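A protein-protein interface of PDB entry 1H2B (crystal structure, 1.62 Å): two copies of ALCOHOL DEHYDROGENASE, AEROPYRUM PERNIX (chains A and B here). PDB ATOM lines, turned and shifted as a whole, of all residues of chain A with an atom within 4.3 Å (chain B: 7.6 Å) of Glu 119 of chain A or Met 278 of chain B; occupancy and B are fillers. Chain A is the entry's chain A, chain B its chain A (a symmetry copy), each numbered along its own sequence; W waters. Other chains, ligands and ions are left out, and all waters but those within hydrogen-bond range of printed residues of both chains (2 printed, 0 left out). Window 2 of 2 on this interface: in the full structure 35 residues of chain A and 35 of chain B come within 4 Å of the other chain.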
ATOM      1  N   ALA A 114      -4.616  25.955  14.279  1.00  0.00           N
ATOM      2  CA  ALA A 114      -3.993  25.709  12.984  1.00  0.00           C
ATOM      3  C   ALA A 114      -4.198  26.884  12.110  1.00  0.00           C
ATOM      4  O   ALA A 114      -3.280  27.304  11.389  1.00  0.00           O
ATOM      5  CB  ALA A 114      -4.561  24.457  12.338  1.00  0.00           C
ATOM      6  N   ALA A 117      -2.075  29.621  12.996  1.00  0.00           N
ATOM      7  CA  ALA A 117      -0.747  29.401  12.490  1.00  0.00           C
ATOM      8  C   ALA A 117      -0.668  29.562  10.967  1.00  0.00           C
ATOM      9  O   ALA A 117       0.429  29.474  10.406  1.00  0.00           O
ATOM     10  CB  ALA A 117      -0.287  28.004  12.921  1.00  0.00           C
ATOM     11  N   GLY A 118      -1.813  29.769  10.311  1.00  0.00           N
ATOM     12  CA  GLY A 118      -1.874  29.935   8.864  1.00  0.00           C
ATOM     13  C   GLY A 118      -2.117  28.677   8.051  1.00  0.00           C
ATOM     14  O   GLY A 118      -1.980  28.731   6.817  1.00  0.00           O
ATOM     15  N   GLU A 119      -2.451  27.576   8.712  1.00  0.00           N
ATOM     16  CA  GLU A 119      -2.595  26.287   7.964  1.00  0.00           C
ATOM     17  C   GLU A 119      -4.045  25.925   7.718  1.00  0.00           C
ATOM     18  O   GLU A 119      -4.644  25.126   8.475  1.00  0.00           O
ATOM     19  CB  GLU A 119      -1.853  25.157   8.673  1.00  0.00           C
ATOM     20  CG  GLU A 119      -0.338  25.368   8.691  1.00  0.00           C
ATOM     21  CD  GLU A 119       0.341  25.034   7.367  1.00  0.00           C
ATOM     22  OE1 GLU A 119      -0.277  25.205   6.311  1.00  0.00           O
ATOM     23  OE2 GLU A 119       1.528  24.659   7.384  1.00  0.00           O
ATOM     24  N   ASP A 120      -4.613  26.499   6.658  1.00  0.00           N
ATOM     25  CA  ASP A 120      -6.057  26.396   6.406  1.00  0.00           C
ATOM     26  C   ASP A 120      -6.499  24.943   6.368  1.00  0.00           C
ATOM     27  O   ASP A 120      -7.620  24.641   6.771  1.00  0.00           O
ATOM     28  CB  ASP A 120      -6.402  27.015   5.046  1.00  0.00           C
ATOM     29  CG  ASP A 120      -6.119  28.505   4.983  1.00  0.00           C
ATOM     30  OD1 ASP A 120      -4.916  28.901   5.074  1.00  0.00           O
ATOM     31  OD2 ASP A 120      -7.041  29.328   4.827  1.00  0.00           O
ATOM     32  N   MET A 121      -5.662  24.035   5.846  1.00  0.00           N
ATOM     33  CA  MET A 121      -6.165  22.675   5.638  1.00  0.00           C
ATOM     34  C   MET A 121      -6.203  21.888   6.907  1.00  0.00           C
ATOM     35  O   MET A 121      -6.675  20.743   6.922  1.00  0.00           O
ATOM     36  CB  MET A 121      -5.311  21.922   4.594  1.00  0.00           C
ATOM     37  CG  MET A 121      -5.304  22.593   3.223  1.00  0.00           C
ATOM     38  SD  MET A 121      -6.946  22.726   2.538  1.00  0.00           S
ATOM     39  CE  MET A 121      -7.526  20.973   2.567  1.00  0.00           C
ATOM     40  N   HIS A 122      -5.677  22.483   7.983  1.00  0.00           N
ATOM     41  CA  HIS A 122      -5.664  21.784   9.291  1.00  0.00           C
ATOM     42  C   HIS A 122      -6.611  22.399  10.286  1.00  0.00           C
ATOM     43  O   HIS A 122      -6.594  22.035  11.466  1.00  0.00           O
ATOM     44  CB  HIS A 122      -4.237  21.661   9.770  1.00  0.00           C
ATOM     45  CG  HIS A 122      -3.466  20.765   8.855  1.00  0.00           C
ATOM     46  ND1 HIS A 122      -3.785  19.437   8.708  1.00  0.00           N
ATOM     47  CD2 HIS A 122      -2.490  21.028   7.952  1.00  0.00           C
ATOM     48  CE1 HIS A 122      -2.994  18.896   7.799  1.00  0.00           C
ATOM     49  NE2 HIS A 122      -2.211  19.847   7.309  1.00  0.00           N
ATOM     50  N   CYS A 123      -7.468  23.262   9.776  1.00  0.00           N
ATOM     51  CA  CYS A 123      -8.480  23.909  10.600  1.00  0.00           C
ATOM     52  C   CYS A 123      -9.501  22.899  11.080  1.00  0.00           C
ATOM     53  O   CYS A 123      -9.945  22.014  10.329  1.00  0.00           O
ATOM     54  CB  CYS A 123      -9.123  25.082   9.868  1.00  0.00           C
ATOM     55  SG  CYS A 123      -7.934  26.413   9.598  1.00  0.00           S
ATOM     56  N   ARG A 175       2.451  23.925  -3.010  1.00  0.00           N
ATOM     57  CA  ARG A 175       2.875  23.511  -1.664  1.00  0.00           C
ATOM     58  C   ARG A 175       3.814  22.320  -1.742  1.00  0.00           C
ATOM     59  O   ARG A 175       4.798  22.241  -1.007  1.00  0.00           O
ATOM     60  CB  ARG A 175       1.665  23.155  -0.807  1.00  0.00           C
ATOM     61  CG  ARG A 175       2.064  22.742   0.623  1.00  0.00           C
ATOM     62  CD  ARG A 175       0.811  22.449   1.382  1.00  0.00           C
ATOM     63  NE  ARG A 175       1.029  22.084   2.794  1.00  0.00           N
ATOM     64  CZ  ARG A 175       1.031  22.923   3.835  1.00  0.00           C
ATOM     65  NH1 ARG A 175       0.917  24.245   3.674  1.00  0.00           N
ATOM     66  NH2 ARG A 175       1.138  22.432   5.073  1.00  0.00           N
ATOM     67  N   ASN A 311      -2.218  26.344   1.743  1.00  0.00           N
ATOM     68  CA  ASN A 311      -2.860  27.343   2.584  1.00  0.00           C
ATOM     69  C   ASN A 311      -3.165  28.633   1.802  1.00  0.00           C
ATOM     70  O   ASN A 311      -2.878  28.750   0.587  1.00  0.00           O
ATOM     71  CB  ASN A 311      -2.052  27.524   3.873  1.00  0.00           C
ATOM     72  CG  ASN A 311      -0.677  28.087   3.657  1.00  0.00           C
ATOM     73  OD1 ASN A 311      -0.474  28.888   2.780  1.00  0.00           O
ATOM     74  ND2 ASN A 311       0.270  27.705   4.514  1.00  0.00           N
ATOM     75  N   THR B 183       9.570  19.841  15.102  1.00  0.00           N
ATOM     76  CA  THR B 183       8.154  20.167  15.142  1.00  0.00           C
ATOM     77  C   THR B 183       7.502  19.995  16.509  1.00  0.00           C
ATOM     78  O   THR B 183       6.264  19.926  16.599  1.00  0.00           O
ATOM     79  CB  THR B 183       7.344  19.394  14.120  1.00  0.00           C
ATOM     80  OG1 THR B 183       7.579  17.968  14.259  1.00  0.00           O
ATOM     81  CG2 THR B 183       7.809  19.724  12.698  1.00  0.00           C
ATOM     82  N   VAL B 255      -0.610  12.094  18.162  1.00  0.00           N
ATOM     83  CA  VAL B 255       0.678  12.642  18.519  1.00  0.00           C
ATOM     84  C   VAL B 255       1.270  13.478  17.380  1.00  0.00           C
ATOM     85  O   VAL B 255       1.049  13.218  16.180  1.00  0.00           O
ATOM     86  CB  VAL B 255       1.700  11.528  19.026  1.00  0.00           C
ATOM     87  CG1 VAL B 255       1.115  10.810  20.259  1.00  0.00           C
ATOM     88  CG2 VAL B 255       2.029  10.495  17.951  1.00  0.00           C
ATOM     89  N   ASN B 256       2.044  14.477  17.763  1.00  0.00           N
ATOM     90  CA  ASN B 256       2.784  15.279  16.787  1.00  0.00           C
ATOM     91  C   ASN B 256       3.929  14.519  16.141  1.00  0.00           C
ATOM     92  O   ASN B 256       4.209  14.700  14.951  1.00  0.00           O
ATOM     93  CB  ASN B 256       3.311  16.532  17.462  1.00  0.00           C
ATOM     94  CG  ASN B 256       2.187  17.336  18.119  1.00  0.00           C
ATOM     95  OD1 ASN B 256       1.592  16.924  19.120  1.00  0.00           O
ATOM     96  ND2 ASN B 256       1.835  18.467  17.504  1.00  0.00           N
ATOM     97  N   VAL B 257       4.608  13.687  16.920  1.00  0.00           N
ATOM     98  CA  VAL B 257       5.688  12.829  16.424  1.00  0.00           C
ATOM     99  C   VAL B 257       5.535  11.478  17.105  1.00  0.00           C
ATOM    100  O   VAL B 257       5.235  11.404  18.298  1.00  0.00           O
ATOM    101  CB  VAL B 257       7.055  13.386  16.803  1.00  0.00           C
ATOM    102  CG1 VAL B 257       8.198  12.454  16.406  1.00  0.00           C
ATOM    103  CG2 VAL B 257       7.271  14.789  16.196  1.00  0.00           C
ATOM    104  N   LEU B 275      -0.473   9.022  14.660  1.00  0.00           N
ATOM    105  CA  LEU B 275      -0.181  10.397  14.251  1.00  0.00           C
ATOM    106  C   LEU B 275      -1.422  11.265  14.127  1.00  0.00           C
ATOM    107  O   LEU B 275      -2.461  10.871  13.562  1.00  0.00           O
ATOM    108  CB  LEU B 275       0.488  10.439  12.850  1.00  0.00           C
ATOM    109  CG  LEU B 275       1.773   9.615  12.722  1.00  0.00           C
ATOM    110  CD1 LEU B 275       2.359   9.665  11.280  1.00  0.00           C
ATOM    111  CD2 LEU B 275       2.848  10.105  13.718  1.00  0.00           C
ATOM    112  N   GLY B 276      -1.254  12.487  14.605  1.00  0.00           N
ATOM    113  CA  GLY B 276      -2.231  13.527  14.360  1.00  0.00           C
ATOM    114  C   GLY B 276      -1.956  14.245  13.054  1.00  0.00           C
ATOM    115  O   GLY B 276      -1.140  13.834  12.241  1.00  0.00           O
ATOM    116  N   ARG B 277      -2.669  15.348  12.873  1.00  0.00           N
ATOM    117  CA  ARG B 277      -2.548  16.109  11.619  1.00  0.00           C
ATOM    118  C   ARG B 277      -1.171  16.708  11.558  1.00  0.00           C
ATOM    119  O   ARG B 277      -0.642  17.284  12.558  1.00  0.00           O
ATOM    120  CB  ARG B 277      -3.604  17.195  11.531  1.00  0.00           C
ATOM    121  CG  ARG B 277      -5.021  16.630  11.453  1.00  0.00           C
ATOM    122  CD  ARG B 277      -6.109  17.666  11.091  1.00  0.00           C
ATOM    123  NE  ARG B 277      -6.074  17.994   9.657  1.00  0.00           N
ATOM    124  CZ  ARG B 277      -6.488  17.214   8.661  1.00  0.00           C
ATOM    125  NH1 ARG B 277      -7.030  16.012   8.875  1.00  0.00           N
ATOM    126  NH2 ARG B 277      -6.383  17.652   7.414  1.00  0.00           N
ATOM    127  N   MET B 278      -0.575  16.622  10.359  1.00  0.00           N
ATOM    128  CA  MET B 278       0.816  17.013  10.139  1.00  0.00           C
ATOM    129  C   MET B 278       1.799  16.250  11.038  1.00  0.00           C
ATOM    130  O   MET B 278       2.967  16.629  11.159  1.00  0.00           O
ATOM    131  CB  MET B 278       1.017  18.541  10.206  1.00  0.00           C
ATOM    132  CG  MET B 278       0.624  19.199   8.900  1.00  0.00           C
ATOM    133  SD  MET B 278       0.920  20.993   8.837  1.00  0.00           S
ATOM    134  CE  MET B 278       2.602  21.101   8.798  1.00  0.00           C
ATOM    135  N   GLY B 279       1.330  15.108  11.539  1.00  0.00           N
ATOM    136  CA  GLY B 279       2.170  14.207  12.351  1.00  0.00           C
ATOM    137  C   GLY B 279       3.323  13.568  11.577  1.00  0.00           C
ATOM    138  O   GLY B 279       3.251  13.411  10.350  1.00  0.00           O
ATOM    139  N   ARG B 280       4.401  13.249  12.290  1.00  0.00           N
ATOM    140  CA  ARG B 280       5.601  12.659  11.691  1.00  0.00           C
ATOM    141  C   ARG B 280       5.962  11.391  12.452  1.00  0.00           C
ATOM    142  O   ARG B 280       6.092  11.403  13.679  1.00  0.00           O
ATOM    143  CB  ARG B 280       6.786  13.599  11.813  1.00  0.00           C
ATOM    144  CG  ARG B 280       6.443  14.988  11.218  1.00  0.00           C
ATOM    145  CD  ARG B 280       7.489  16.038  11.527  1.00  0.00           C
ATOM    146  NE  ARG B 280       8.842  15.595  11.204  1.00  0.00           N
ATOM    147  CZ  ARG B 280       9.932  15.927  11.888  1.00  0.00           C
ATOM    148  NH1 ARG B 280       9.850  16.746  12.952  1.00  0.00           N
ATOM    149  NH2 ARG B 280      11.103  15.490  11.509  1.00  0.00           N
ATOM    150  N   LEU B 281       6.181  10.317  11.703  1.00  0.00           N
ATOM    151  CA  LEU B 281       6.676   9.066  12.285  1.00  0.00           C
ATOM    152  C   LEU B 281       8.134   8.939  11.905  1.00  0.00           C
ATOM    153  O   LEU B 281       8.496   8.902  10.719  1.00  0.00           O
ATOM    154  CB  LEU B 281       5.911   7.881  11.675  1.00  0.00           C
ATOM    155  CG  LEU B 281       6.404   6.473  11.996  1.00  0.00           C
ATOM    156  CD1 LEU B 281       6.523   6.162  13.497  1.00  0.00           C
ATOM    157  CD2 LEU B 281       5.462   5.468  11.281  1.00  0.00           C
ATOM    158  N   VAL B 297      -2.317   9.301   4.129  1.00  0.00           N
ATOM    159  CA  VAL B 297      -1.073  10.077   4.082  1.00  0.00           C
ATOM    160  C   VAL B 297      -1.416  11.526   3.714  1.00  0.00           C
ATOM    161  O   VAL B 297      -0.932  12.453   4.369  1.00  0.00           O
ATOM    162  CB  VAL B 297      -0.076   9.497   3.053  1.00  0.00           C
ATOM    163  CG1 VAL B 297       1.144  10.416   2.859  1.00  0.00           C
ATOM    164  CG2 VAL B 297       0.428   8.134   3.538  1.00  0.00           C
ATOM    165  N   SER B 299      -4.612  12.997   3.533  1.00  0.00           N
ATOM    166  CA  SER B 299      -5.701  13.695   4.248  1.00  0.00           C
ATOM    167  C   SER B 299      -5.266  14.179   5.633  1.00  0.00           C
ATOM    168  O   SER B 299      -5.796  15.194   6.092  1.00  0.00           O
ATOM    169  CB  SER B 299      -6.989  12.873   4.310  1.00  0.00           C
ATOM    170  OG  SER B 299      -6.725  11.689   4.986  1.00  0.00           O
ATOM    171  N   SER B 300      -4.328  13.479   6.273  1.00  0.00           N
ATOM    172  CA  SER B 300      -3.727  13.914   7.530  1.00  0.00           C
ATOM    173  C   SER B 300      -2.462  14.741   7.307  1.00  0.00           C
ATOM    174  O   SER B 300      -1.947  15.327   8.264  1.00  0.00           O
ATOM    175  CB  SER B 300      -3.355  12.672   8.371  1.00  0.00           C
ATOM    176  OG  SER B 300      -4.511  12.102   8.914  1.00  0.00           O
ATOM    177  N   GLU B 301      -1.952  14.769   6.065  1.00  0.00           N
ATOM    178  CA  GLU B 301      -0.652  15.391   5.721  1.00  0.00           C
ATOM    179  C   GLU B 301       0.495  14.918   6.649  1.00  0.00           C
ATOM    180  O   GLU B 301       1.201  15.726   7.288  1.00  0.00           O
ATOM    181  CB  GLU B 301      -0.747  16.919   5.678  1.00  0.00           C
ATOM    182  CG  GLU B 301       0.265  17.481   4.679  1.00  0.00           C
ATOM    183  CD  GLU B 301       0.214  18.981   4.444  1.00  0.00           C
ATOM    184  OE1 GLU B 301      -0.387  19.720   5.255  1.00  0.00           O
ATOM    185  OE2 GLU B 301       0.831  19.410   3.427  1.00  0.00           O
ATOM    186  N   VAL B 302       0.639  13.596   6.756  1.00  0.00           N
ATOM    187  CA  VAL B 302       1.663  13.024   7.591  1.00  0.00           C
ATOM    188  C   VAL B 302       2.900  12.601   6.815  1.00  0.00           C
ATOM    189  O   VAL B 302       2.884  12.487   5.585  1.00  0.00           O
ATOM    190  CB  VAL B 302       1.163  11.803   8.395  1.00  0.00           C
ATOM    191  CG1 VAL B 302       0.096  12.240   9.403  1.00  0.00           C
ATOM    192  CG2 VAL B 302       0.571  10.776   7.465  1.00  0.00           C
ATOM    193  N   SER B 303       3.988  12.350   7.545  1.00  0.00           N
ATOM    194  CA  SER B 303       5.219  11.908   6.927  1.00  0.00           C
ATOM    195  C   SER B 303       5.793  10.745   7.712  1.00  0.00           C
ATOM    196  O   SER B 303       5.550  10.589   8.927  1.00  0.00           O
ATOM    197  CB  SER B 303       6.239  13.043   6.858  1.00  0.00           C
ATOM    198  OG  SER B 303       6.536  13.509   8.150  1.00  0.00           O
ATOM    199  N   GLU B 305       9.609   9.084   8.229  1.00  0.00           N
ATOM    200  CA  GLU B 305      10.979   9.590   8.015  1.00  0.00           C
ATOM    201  C   GLU B 305      11.969   8.621   8.627  1.00  0.00           C
ATOM    202  O   GLU B 305      11.992   8.482   9.858  1.00  0.00           O
ATOM    203  CB  GLU B 305      11.162  10.978   8.673  1.00  0.00           C
ATOM    204  CG  GLU B 305      10.146  12.001   8.126  1.00  0.00           C
ATOM    205  CD  GLU B 305      10.146  13.322   8.849  1.00  0.00           C
ATOM    206  OE1 GLU B 305      11.221  13.793   9.226  1.00  0.00           O
ATOM    207  OE2 GLU B 305       9.054  13.873   8.993  1.00  0.00           O
HETATM  208  O   HOH W   1       3.021  19.828   5.600  1.00  0.00           O
HETATM  209  O   HOH W   2      -2.020  21.738   3.986  1.00  0.00           O
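O of Ser 300 of chain B is in hydrogen-bond range of N of Met 278 of chain B (2.8 Å).
The guanidinium group (NH2) of Arg 277 of chain B lies within hydrogen-bond range of the backbone carbonyl oxygen (O) of Ser 299 of chain B.
NH1 of Arg 175 of chain A is in salt-bridge range of OE1 of Glu 119 of chain A (3.0 Å).
OE1 of Glu 119 of chain A lies within hydrogen-bond range of ND2 of Asn 311 of chain A (3.1 Å).
N of Glu 119 of chain A lies within hydrogen-bond range of O of Ala 114 of chain A.
OE2 of Glu 119 of chain A touches CE of Met 278 of chain B, 3.98 Å away.
Ser 300 of chain B touches His 122 of chain A (O to CE1, 3.7 Å).
Of the 10 printed residues of chain A, 4 touch a printed residue of chain B.
Printed residues of chain A that touch a printed residue of chain B: Glu 119, Met 121, His 122 and Arg 175.
Hydrophobic or aromatic side chains of chain A that line the printed part of chain B: His 122.
Of the 18 printed residues of chain B, 4 touch a printed residue of chain A.
Printed residues of chain B that touch a printed residue of chain A: Arg 277, Met 278, Ser 300 and Glu 301.
Among the printed residues, Asp or Glu carboxylates within 4 Å of a Lys or Arg side-chain nitrogen of the other chain: Arg 175 of chain A with Glu 301 of chain B.
No position is printed for both chains.
Water W2 bridges OE1 of Glu 301 of chain B (2.9 Å) and NE of Arg 175 of chain A (3.3 Å).
Water W1 lies within hydrogen-bond range of the side-chain carboxylate of Glu 301 of chain B and the guanidinium group of Arg 175 of chain A.
The backbone carbonyl oxygen of Met 121 of chain A sits at hydrogen-bond distance from the guanidinium group of Arg 277 of chain B, 3.1 Å away.
A ring nitrogen (NE2) of His 122 of chain A lies close to the side-chain sulfur of Met 278 of chain B (3.7 Å).
The side-chain carboxylate (OE2) of Glu 301 of chain B lies within salt-bridge range of the guanidinium group (NE) of Arg 175 of chain A, 2.8 Å away.
A ring nitrogen (ND1) of His 122 of chain A is in hydrogen-bond range of the guanidinium group of Arg 277 of chain B (2.9 Å).
NE2 of His 122 of chain A is in hydrogen-bond range of OE1 of Glu 301 of chain B.
Printed residues of chain B within 4 Å of Glu 119 of chain A: Met 278 (3.98 Å).
Of the printed residues of chain A, Met 278 of chain B touches Glu 119 (3.98 Å) and His 122 (3.3 Å).
No residue of chain B comes within 4 Å of Gly 118 of chain A.
Of the printed residues of chain B, Arg 175 of chain A touches Glu 301.
Printed residues of chain A within 4 Å of Arg 277 of chain B: Met 121 (3.1 Å) and His 122 (2.9 Å).
Val 302 of chain B touches none of the printed residues of chain A.
The nearest printed residue of chain A that does not touch Met 278 of chain B is Arg 175 of chain A (4.04 Å).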
